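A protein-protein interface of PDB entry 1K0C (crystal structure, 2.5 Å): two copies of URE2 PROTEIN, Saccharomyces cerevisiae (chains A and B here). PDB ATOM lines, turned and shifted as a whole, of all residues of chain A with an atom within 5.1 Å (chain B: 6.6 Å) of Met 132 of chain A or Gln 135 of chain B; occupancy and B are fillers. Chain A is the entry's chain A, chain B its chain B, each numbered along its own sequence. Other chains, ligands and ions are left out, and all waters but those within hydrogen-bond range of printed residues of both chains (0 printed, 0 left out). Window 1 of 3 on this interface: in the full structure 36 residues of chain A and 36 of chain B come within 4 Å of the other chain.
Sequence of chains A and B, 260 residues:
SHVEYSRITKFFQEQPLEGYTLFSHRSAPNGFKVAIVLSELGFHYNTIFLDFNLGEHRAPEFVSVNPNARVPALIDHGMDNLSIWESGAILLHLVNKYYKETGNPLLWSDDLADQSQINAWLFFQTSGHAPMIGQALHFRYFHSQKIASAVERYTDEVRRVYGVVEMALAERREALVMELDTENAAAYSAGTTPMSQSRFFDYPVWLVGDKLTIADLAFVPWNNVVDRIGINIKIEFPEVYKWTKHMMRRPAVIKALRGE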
ATOM      1  N   GLY A 128      25.503  -2.926 -20.138  1.00  0.00           N
ATOM      2  CA  GLY A 128      26.931  -2.727 -20.313  1.00  0.00           C
ATOM      3  C   GLY A 128      27.378  -2.109 -21.627  1.00  0.00           C
ATOM      4  O   GLY A 128      28.530  -1.702 -21.761  1.00  0.00           O
ATOM      5  N   HIS A 129      26.477  -2.027 -22.595  1.00  0.00           N
ATOM      6  CA  HIS A 129      26.804  -1.475 -23.904  1.00  0.00           C
ATOM      7  C   HIS A 129      26.248  -0.057 -24.036  1.00  0.00           C
ATOM      8  O   HIS A 129      27.001   0.917 -24.049  1.00  0.00           O
ATOM      9  CB  HIS A 129      26.216  -2.382 -24.991  1.00  0.00           C
ATOM     10  CG  HIS A 129      26.781  -2.157 -26.361  1.00  0.00           C
ATOM     11  ND1 HIS A 129      25.983  -2.015 -27.479  1.00  0.00           N
ATOM     12  CD2 HIS A 129      28.059  -2.101 -26.803  1.00  0.00           C
ATOM     13  CE1 HIS A 129      26.746  -1.880 -28.549  1.00  0.00           C
ATOM     14  NE2 HIS A 129      28.011  -1.929 -28.167  1.00  0.00           N
ATOM     15  N   ALA A 130      24.927   0.056 -24.100  1.00  0.00           N
ATOM     16  CA  ALA A 130      24.270   1.354 -24.262  1.00  0.00           C
ATOM     17  C   ALA A 130      24.633   2.411 -23.228  1.00  0.00           C
ATOM     18  O   ALA A 130      24.815   3.584 -23.565  1.00  0.00           O
ATOM     19  CB  ALA A 130      22.757   1.171 -24.303  1.00  0.00           C
ATOM     20  N   PRO A 131      24.739   2.024 -21.951  1.00  0.00           N
ATOM     21  CA  PRO A 131      25.082   3.038 -20.952  1.00  0.00           C
ATOM     22  C   PRO A 131      26.478   3.629 -21.176  1.00  0.00           C
ATOM     23  O   PRO A 131      26.694   4.835 -21.011  1.00  0.00           O
ATOM     24  CB  PRO A 131      24.985   2.266 -19.635  1.00  0.00           C
ATOM     25  CG  PRO A 131      24.034   1.147 -19.947  1.00  0.00           C
ATOM     26  CD  PRO A 131      24.481   0.724 -21.311  1.00  0.00           C
ATOM     27  N   MET A 132      27.420   2.773 -21.558  1.00  0.00           N
ATOM     28  CA  MET A 132      28.797   3.196 -21.790  1.00  0.00           C
ATOM     29  C   MET A 132      28.932   4.052 -23.046  1.00  0.00           C
ATOM     30  O   MET A 132      29.720   5.005 -23.082  1.00  0.00           O
ATOM     31  CB  MET A 132      29.702   1.969 -21.872  1.00  0.00           C
ATOM     32  CG  MET A 132      29.655   1.104 -20.612  1.00  0.00           C
ATOM     33  SD  MET A 132      30.201   1.990 -19.118  1.00  0.00           S
ATOM     34  CE  MET A 132      28.670   2.613 -18.487  1.00  0.00           C
ATOM     35  N   ILE A 133      28.162   3.719 -24.077  1.00  0.00           N
ATOM     36  CA  ILE A 133      28.188   4.502 -25.300  1.00  0.00           C
ATOM     37  C   ILE A 133      27.644   5.887 -24.931  1.00  0.00           C
ATOM     38  O   ILE A 133      28.259   6.916 -25.235  1.00  0.00           O
ATOM     39  CB  ILE A 133      27.301   3.860 -26.387  1.00  0.00           C
ATOM     40  CG1 ILE A 133      27.954   2.567 -26.882  1.00  0.00           C
ATOM     41  CG2 ILE A 133      27.094   4.830 -27.536  1.00  0.00           C
ATOM     42  CD1 ILE A 133      27.027   1.674 -27.715  1.00  0.00           C
ATOM     43  N   GLY A 134      26.501   5.899 -24.254  1.00  0.00           N
ATOM     44  CA  GLY A 134      25.892   7.150 -23.832  1.00  0.00           C
ATOM     45  C   GLY A 134      26.801   8.044 -23.006  1.00  0.00           C
ATOM     46  O   GLY A 134      26.799   9.270 -23.184  1.00  0.00           O
ATOM     47  N   GLN A 135      27.576   7.453 -22.097  1.00  0.00           N
ATOM     48  CA  GLN A 135      28.488   8.244 -21.274  1.00  0.00           C
ATOM     49  C   GLN A 135      29.615   8.760 -22.150  1.00  0.00           C
ATOM     50  O   GLN A 135      30.059   9.906 -22.007  1.00  0.00           O
ATOM     51  CB  GLN A 135      29.080   7.409 -20.131  1.00  0.00           C
ATOM     52  CG  GLN A 135      28.109   7.054 -19.001  1.00  0.00           C
ATOM     53  CD  GLN A 135      26.808   7.812 -19.092  1.00  0.00           C
ATOM     54  OE1 GLN A 135      25.890   7.396 -19.794  1.00  0.00           O
ATOM     55  NE2 GLN A 135      26.725   8.940 -18.395  1.00  0.00           N
ATOM     56  N   ALA A 136      30.071   7.909 -23.065  1.00  0.00           N
ATOM     57  CA  ALA A 136      31.147   8.285 -23.971  1.00  0.00           C
ATOM     58  C   ALA A 136      30.716   9.482 -24.817  1.00  0.00           C
ATOM     59  O   ALA A 136      31.503  10.393 -25.063  1.00  0.00           O
ATOM     60  CB  ALA A 136      31.525   7.104 -24.860  1.00  0.00           C
ATOM     61  N   LEU A 137      29.460   9.488 -25.249  1.00  0.00           N
ATOM     62  CA  LEU A 137      28.951  10.595 -26.046  1.00  0.00           C
ATOM     63  C   LEU A 137      28.897  11.867 -25.218  1.00  0.00           C
ATOM     64  O   LEU A 137      29.329  12.935 -25.657  1.00  0.00           O
ATOM     65  CB  LEU A 137      27.547  10.284 -26.566  1.00  0.00           C
ATOM     66  CG  LEU A 137      27.474   9.329 -27.756  1.00  0.00           C
ATOM     67  CD1 LEU A 137      26.040   8.840 -27.943  1.00  0.00           C
ATOM     68  CD2 LEU A 137      27.988  10.038 -29.003  1.00  0.00           C
ATOM     69  N   ARG A 153      37.862   6.762 -20.544  1.00  0.00           N
ATOM     70  CA  ARG A 153      37.213   5.779 -19.694  1.00  0.00           C
ATOM     71  C   ARG A 153      36.104   5.039 -20.440  1.00  0.00           C
ATOM     72  O   ARG A 153      36.098   3.808 -20.512  1.00  0.00           O
ATOM     73  CB  ARG A 153      36.625   6.456 -18.448  1.00  0.00           C
ATOM     74  CG  ARG A 153      35.831   5.504 -17.543  1.00  0.00           C
ATOM     75  CD  ARG A 153      35.436   6.136 -16.198  1.00  0.00           C
ATOM     76  NE  ARG A 153      34.504   5.278 -15.469  1.00  0.00           N
ATOM     77  CZ  ARG A 153      34.814   4.087 -14.957  1.00  0.00           C
ATOM     78  NH1 ARG A 153      36.046   3.607 -15.078  1.00  0.00           N
ATOM     79  NH2 ARG A 153      33.882   3.354 -14.359  1.00  0.00           N
ATOM     80  N   TYR A 154      35.177   5.793 -21.017  1.00  0.00           N
ATOM     81  CA  TYR A 154      34.060   5.186 -21.718  1.00  0.00           C
ATOM     82  C   TYR A 154      34.328   4.605 -23.108  1.00  0.00           C
ATOM     83  O   TYR A 154      33.747   3.582 -23.479  1.00  0.00           O
ATOM     84  CB  TYR A 154      32.917   6.186 -21.736  1.00  0.00           C
ATOM     85  CG  TYR A 154      32.481   6.484 -20.325  1.00  0.00           C
ATOM     86  CD1 TYR A 154      32.750   7.716 -19.730  1.00  0.00           C
ATOM     87  CD2 TYR A 154      31.882   5.487 -19.544  1.00  0.00           C
ATOM     88  CE1 TYR A 154      32.434   7.948 -18.387  1.00  0.00           C
ATOM     89  CE2 TYR A 154      31.568   5.706 -18.202  1.00  0.00           C
ATOM     90  CZ  TYR A 154      31.846   6.937 -17.634  1.00  0.00           C
ATOM     91  OH  TYR A 154      31.530   7.147 -16.317  1.00  0.00           O
ATOM     92  N   GLU A 157      35.951   1.227 -22.503  1.00  0.00           N
ATOM     93  CA  GLU A 157      34.988   0.245 -22.047  1.00  0.00           C
ATOM     94  C   GLU A 157      34.129  -0.268 -23.189  1.00  0.00           C
ATOM     95  O   GLU A 157      33.891  -1.473 -23.290  1.00  0.00           O
ATOM     96  CB  GLU A 157      34.111   0.832 -20.940  1.00  0.00           C
ATOM     97  CG  GLU A 157      33.071  -0.143 -20.382  1.00  0.00           C
ATOM     98  CD  GLU A 157      33.671  -1.449 -19.837  1.00  0.00           C
ATOM     99  OE1 GLU A 157      32.880  -2.344 -19.474  1.00  0.00           O
ATOM    100  OE2 GLU A 157      34.912  -1.586 -19.765  1.00  0.00           O
ATOM    101  N   VAL A 158      33.671   0.643 -24.046  1.00  0.00           N
ATOM    102  CA  VAL A 158      32.851   0.267 -25.194  1.00  0.00           C
ATOM    103  C   VAL A 158      33.655  -0.641 -26.117  1.00  0.00           C
ATOM    104  O   VAL A 158      33.121  -1.592 -26.700  1.00  0.00           O
ATOM    105  CB  VAL A 158      32.392   1.493 -26.008  1.00  0.00           C
ATOM    106  CG1 VAL A 158      31.622   1.023 -27.238  1.00  0.00           C
ATOM    107  CG2 VAL A 158      31.512   2.398 -25.154  1.00  0.00           C
ATOM    108  N   ALA B 130      22.095   0.465 -11.202  1.00  0.00           N
ATOM    109  CA  ALA B 130      23.451  -0.036 -10.991  1.00  0.00           C
ATOM    110  C   ALA B 130      24.583   0.688 -11.712  1.00  0.00           C
ATOM    111  O   ALA B 130      25.536   1.132 -11.073  1.00  0.00           O
ATOM    112  CB  ALA B 130      23.509  -1.535 -11.316  1.00  0.00           C
ATOM    113  N   PRO B 131      24.509   0.814 -13.048  1.00  0.00           N
ATOM    114  CA  PRO B 131      25.604   1.502 -13.743  1.00  0.00           C
ATOM    115  C   PRO B 131      25.908   2.892 -13.187  1.00  0.00           C
ATOM    116  O   PRO B 131      27.073   3.267 -13.027  1.00  0.00           O
ATOM    117  CB  PRO B 131      25.123   1.539 -15.199  1.00  0.00           C
ATOM    118  CG  PRO B 131      24.304   0.286 -15.309  1.00  0.00           C
ATOM    119  CD  PRO B 131      23.508   0.317 -14.013  1.00  0.00           C
ATOM    120  N   MET B 132      24.859   3.642 -12.876  1.00  0.00           N
ATOM    121  CA  MET B 132      25.017   4.991 -12.358  1.00  0.00           C
ATOM    122  C   MET B 132      25.678   5.024 -10.985  1.00  0.00           C
ATOM    123  O   MET B 132      26.568   5.842 -10.741  1.00  0.00           O
ATOM    124  CB  MET B 132      23.660   5.692 -12.333  1.00  0.00           C
ATOM    125  CG  MET B 132      23.031   5.802 -13.720  1.00  0.00           C
ATOM    126  SD  MET B 132      23.960   6.848 -14.908  1.00  0.00           S
ATOM    127  CE  MET B 132      25.178   5.725 -15.547  1.00  0.00           C
ATOM    128  N   ILE B 133      25.255   4.144 -10.086  1.00  0.00           N
ATOM    129  CA  ILE B 133      25.868   4.107  -8.766  1.00  0.00           C
ATOM    130  C   ILE B 133      27.357   3.814  -8.973  1.00  0.00           C
ATOM    131  O   ILE B 133      28.224   4.379  -8.303  1.00  0.00           O
ATOM    132  CB  ILE B 133      25.237   3.006  -7.886  1.00  0.00           C
ATOM    133  CG1 ILE B 133      23.755   3.311  -7.665  1.00  0.00           C
ATOM    134  CG2 ILE B 133      25.957   2.914  -6.550  1.00  0.00           C
ATOM    135  CD1 ILE B 133      23.016   2.236  -6.875  1.00  0.00           C
ATOM    136  N   GLY B 134      27.645   2.931  -9.920  1.00  0.00           N
ATOM    137  CA  GLY B 134      29.023   2.590 -10.217  1.00  0.00           C
ATOM    138  C   GLY B 134      29.828   3.751 -10.783  1.00  0.00           C
ATOM    139  O   GLY B 134      30.995   3.910 -10.437  1.00  0.00           O
ATOM    140  N   GLN B 135      29.234   4.568 -11.647  1.00  0.00           N
ATOM    141  CA  GLN B 135      29.988   5.692 -12.202  1.00  0.00           C
ATOM    142  C   GLN B 135      30.177   6.768 -11.141  1.00  0.00           C
ATOM    143  O   GLN B 135      31.164   7.507 -11.163  1.00  0.00           O
ATOM    144  CB  GLN B 135      29.287   6.293 -13.431  1.00  0.00           C
ATOM    145  CG  GLN B 135      28.977   5.286 -14.537  1.00  0.00           C
ATOM    146  CD  GLN B 135      30.123   4.303 -14.817  1.00  0.00           C
ATOM    147  OE1 GLN B 135      29.924   3.085 -14.804  1.00  0.00           O
ATOM    148  NE2 GLN B 135      31.313   4.826 -15.079  1.00  0.00           N
ATOM    149  N   ALA B 136      29.235   6.857 -10.208  1.00  0.00           N
ATOM    150  CA  ALA B 136      29.341   7.843  -9.145  1.00  0.00           C
ATOM    151  C   ALA B 136      30.525   7.441  -8.272  1.00  0.00           C
ATOM    152  O   ALA B 136      31.465   8.220  -8.064  1.00  0.00           O
ATOM    153  CB  ALA B 136      28.069   7.872  -8.327  1.00  0.00           C
ATOM    154  N   LEU B 137      30.479   6.210  -7.778  1.00  0.00           N
ATOM    155  CA  LEU B 137      31.541   5.682  -6.937  1.00  0.00           C
ATOM    156  C   LEU B 137      32.883   5.845  -7.613  1.00  0.00           C
ATOM    157  O   LEU B 137      33.880   6.172  -6.961  1.00  0.00           O
ATOM    158  CB  LEU B 137      31.303   4.198  -6.653  1.00  0.00           C
ATOM    159  CG  LEU B 137      30.101   3.904  -5.752  1.00  0.00           C
ATOM    160  CD1 LEU B 137      29.716   2.437  -5.864  1.00  0.00           C
ATOM    161  CD2 LEU B 137      30.439   4.294  -4.302  1.00  0.00           C
ATOM    162  N   HIS B 138      32.910   5.632  -8.926  1.00  0.00           N
ATOM    163  CA  HIS B 138      34.167   5.722  -9.652  1.00  0.00           C
ATOM    164  C   HIS B 138      34.836   7.078  -9.587  1.00  0.00           C
ATOM    165  O   HIS B 138      36.002   7.178  -9.234  1.00  0.00           O
ATOM    166  CB  HIS B 138      33.999   5.341 -11.118  1.00  0.00           C
ATOM    167  CG  HIS B 138      35.280   5.407 -11.885  1.00  0.00           C
ATOM    168  ND1 HIS B 138      36.288   4.481 -11.725  1.00  0.00           N
ATOM    169  CD2 HIS B 138      35.762   6.344 -12.735  1.00  0.00           C
ATOM    170  CE1 HIS B 138      37.337   4.845 -12.441  1.00  0.00           C
ATOM    171  NE2 HIS B 138      37.043   5.973 -13.062  1.00  0.00           N
ATOM    172  N   PHE B 139      34.111   8.129  -9.943  1.00  0.00           N
ATOM    173  CA  PHE B 139      34.701   9.454  -9.920  1.00  0.00           C
ATOM    174  C   PHE B 139      34.918   9.943  -8.501  1.00  0.00           C
ATOM    175  O   PHE B 139      35.932  10.558  -8.197  1.00  0.00           O
ATOM    176  CB  PHE B 139      33.846  10.424 -10.738  1.00  0.00           C
ATOM    177  CG  PHE B 139      33.882  10.137 -12.216  1.00  0.00           C
ATOM    178  CD1 PHE B 139      32.930   9.310 -12.805  1.00  0.00           C
ATOM    179  CD2 PHE B 139      34.923  10.629 -13.007  1.00  0.00           C
ATOM    180  CE1 PHE B 139      33.012   8.970 -14.153  1.00  0.00           C
ATOM    181  CE2 PHE B 139      35.021  10.296 -14.356  1.00  0.00           C
ATOM    182  CZ  PHE B 139      34.063   9.464 -14.932  1.00  0.00           C
ATOM    183  N   ARG B 140      33.983   9.639  -7.618  1.00  0.00           N
ATOM    184  CA  ARG B 140      34.121  10.043  -6.231  1.00  0.00           C
ATOM    185  C   ARG B 140      35.365   9.420  -5.600  1.00  0.00           C
ATOM    186  O   ARG B 140      36.077  10.079  -4.841  1.00  0.00           O
ATOM    187  CB  ARG B 140      32.894   9.597  -5.441  1.00  0.00           C
ATOM    188  CG  ARG B 140      32.962   9.907  -3.963  1.00  0.00           C
ATOM    189  CD  ARG B 140      32.624  11.357  -3.687  1.00  0.00           C
ATOM    190  NE  ARG B 140      32.606  11.651  -2.257  1.00  0.00           N
ATOM    191  CZ  ARG B 140      33.692  11.708  -1.490  1.00  0.00           C
ATOM    192  NH1 ARG B 140      33.578  11.979  -0.195  1.00  0.00           N
ATOM    193  NH2 ARG B 140      34.896  11.506  -2.016  1.00  0.00           N
ATOM    194  N   ALA B 150      31.663  15.444 -12.773  1.00  0.00           N
ATOM    195  CA  ALA B 150      31.307  14.064 -13.086  1.00  0.00           C
ATOM    196  C   ALA B 150      30.638  13.448 -11.855  1.00  0.00           C
ATOM    197  O   ALA B 150      29.615  12.770 -11.971  1.00  0.00           O
ATOM    198  CB  ALA B 150      32.559  13.259 -13.480  1.00  0.00           C
ATOM    199  N   VAL B 151      31.216  13.697 -10.680  1.00  0.00           N
ATOM    200  CA  VAL B 151      30.671  13.182  -9.428  1.00  0.00           C
ATOM    201  C   VAL B 151      29.251  13.710  -9.281  1.00  0.00           C
ATOM    202  O   VAL B 151      28.328  12.960  -8.977  1.00  0.00           O
ATOM    203  CB  VAL B 151      31.517  13.644  -8.195  1.00  0.00           C
ATOM    204  CG1 VAL B 151      30.935  13.066  -6.905  1.00  0.00           C
ATOM    205  CG2 VAL B 151      32.976  13.202  -8.348  1.00  0.00           C
ATOM    206  N   TYR B 154      26.628  11.966 -11.884  1.00  0.00           N
ATOM    207  CA  TYR B 154      26.130  10.661 -11.481  1.00  0.00           C
ATOM    208  C   TYR B 154      25.410  10.633 -10.144  1.00  0.00           C
ATOM    209  O   TYR B 154      24.451   9.878  -9.965  1.00  0.00           O
ATOM    210  CB  TYR B 154      27.270   9.643 -11.524  1.00  0.00           C
ATOM    211  CG  TYR B 154      27.777   9.497 -12.931  1.00  0.00           C
ATOM    212  CD1 TYR B 154      28.937  10.139 -13.345  1.00  0.00           C
ATOM    213  CD2 TYR B 154      27.016   8.818 -13.894  1.00  0.00           C
ATOM    214  CE1 TYR B 154      29.331  10.121 -14.685  1.00  0.00           C
ATOM    215  CE2 TYR B 154      27.399   8.795 -15.242  1.00  0.00           C
ATOM    216  CZ  TYR B 154      28.554   9.449 -15.627  1.00  0.00           C
ATOM    217  OH  TYR B 154      28.920   9.454 -16.952  1.00  0.00           O
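Hydrophobic or aromatic side chains of chain A within 4 Å of the printed part of chain B: Met 132 and Tyr 154.
Hydrophobic or aromatic side chains of chain B that line the printed part of chain A: His 138, Phe 139 and Tyr 154.
Among the printed residues, pairs that only touch across the chains: Met 132 of chain A with Gln 135 of chain B (3.9 Å), Arg 153 of chain A with Phe 139 of chain B (3.8 Å), Tyr 154 of chain A with Phe 139 of chain B (3.2 Å) and Tyr 154 of chain A with Tyr 154 of chain B (3.5 Å).
The side-chain amide oxygen of Gln 135 of chain A lies close to the backbone carbonyl oxygen of Pro 131 of chain A (2.9 Å).
The backbone carbonyl oxygen of Pro 131 of chain B sits close to the side-chain amide oxygen of Gln 135 of chain B, 3.4 Å away.
Of chain B, only Gln 135 comes within 4 Å of Met 132 of chain A.
Printed residues of chain B within 4 Å of Arg 153 of chain A: Gln 135, His 138 and Phe 139.
Of the printed residues of chain B, Tyr 154 of chain A touches Gln 135, Phe 139 and Tyr 154.
Met 132 of chain B touches none of the printed residues of chain A.
Of chain A, only Met 132 (3.9 Å), Arg 153 (3.0 Å) and Tyr 154 (2.6 Å) come within 4 Å of Gln 135 of chain B.
Of the printed residues of chain A, His 138 of chain B touches Arg 153.
Of the printed residues of chain A, Tyr 154 of chain B touches Gln 135 (2.7 Å) and Tyr 154 (3.5 Å).
The nearest residue of chain B that does not touch Met 132 of chain A is Pro 131 of chain B (5.0 Å).
The nearest printed residue of chain B that does not touch Arg 153 of chain A is Gly 134 of chain B (4.9 Å).
NE2 of Gln 135 of chain A lies within hydrogen-bond range of OH of Tyr 154 of chain B, at 2.7 Å.
The side-chain amide nitrogen of Gln 135 of chain B lies close to the guanidinium group of Arg 153 of chain A (3.0 Å).
A ring nitrogen (NE2) of His 138 of chain B lies close to the guanidinium group of Arg 153 of chain A.
The side-chain hydroxyl of Tyr 154 of chain A lies within hydrogen-bond range of the side-chain amide nitrogen of Gln 135 of chain B (2.6 Å).
Met 132 of chain A touches Gln 135 of chain B, but with the chains exchanged Gln 135 of chain A does not touch Met 132 of chain B (4.4 Å).
Gln 135 of chain A touches Tyr 154 of chain B, and with the chains exchanged Tyr 154 of chain A touches Gln 135 of chain B.
Tyr 154 of chain A touches its own counterpart, Tyr 154 of chain B.
Of the 8 pairs that touch across the chains among the printed residues, 3 have their exchanged pair printed and touching as well.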
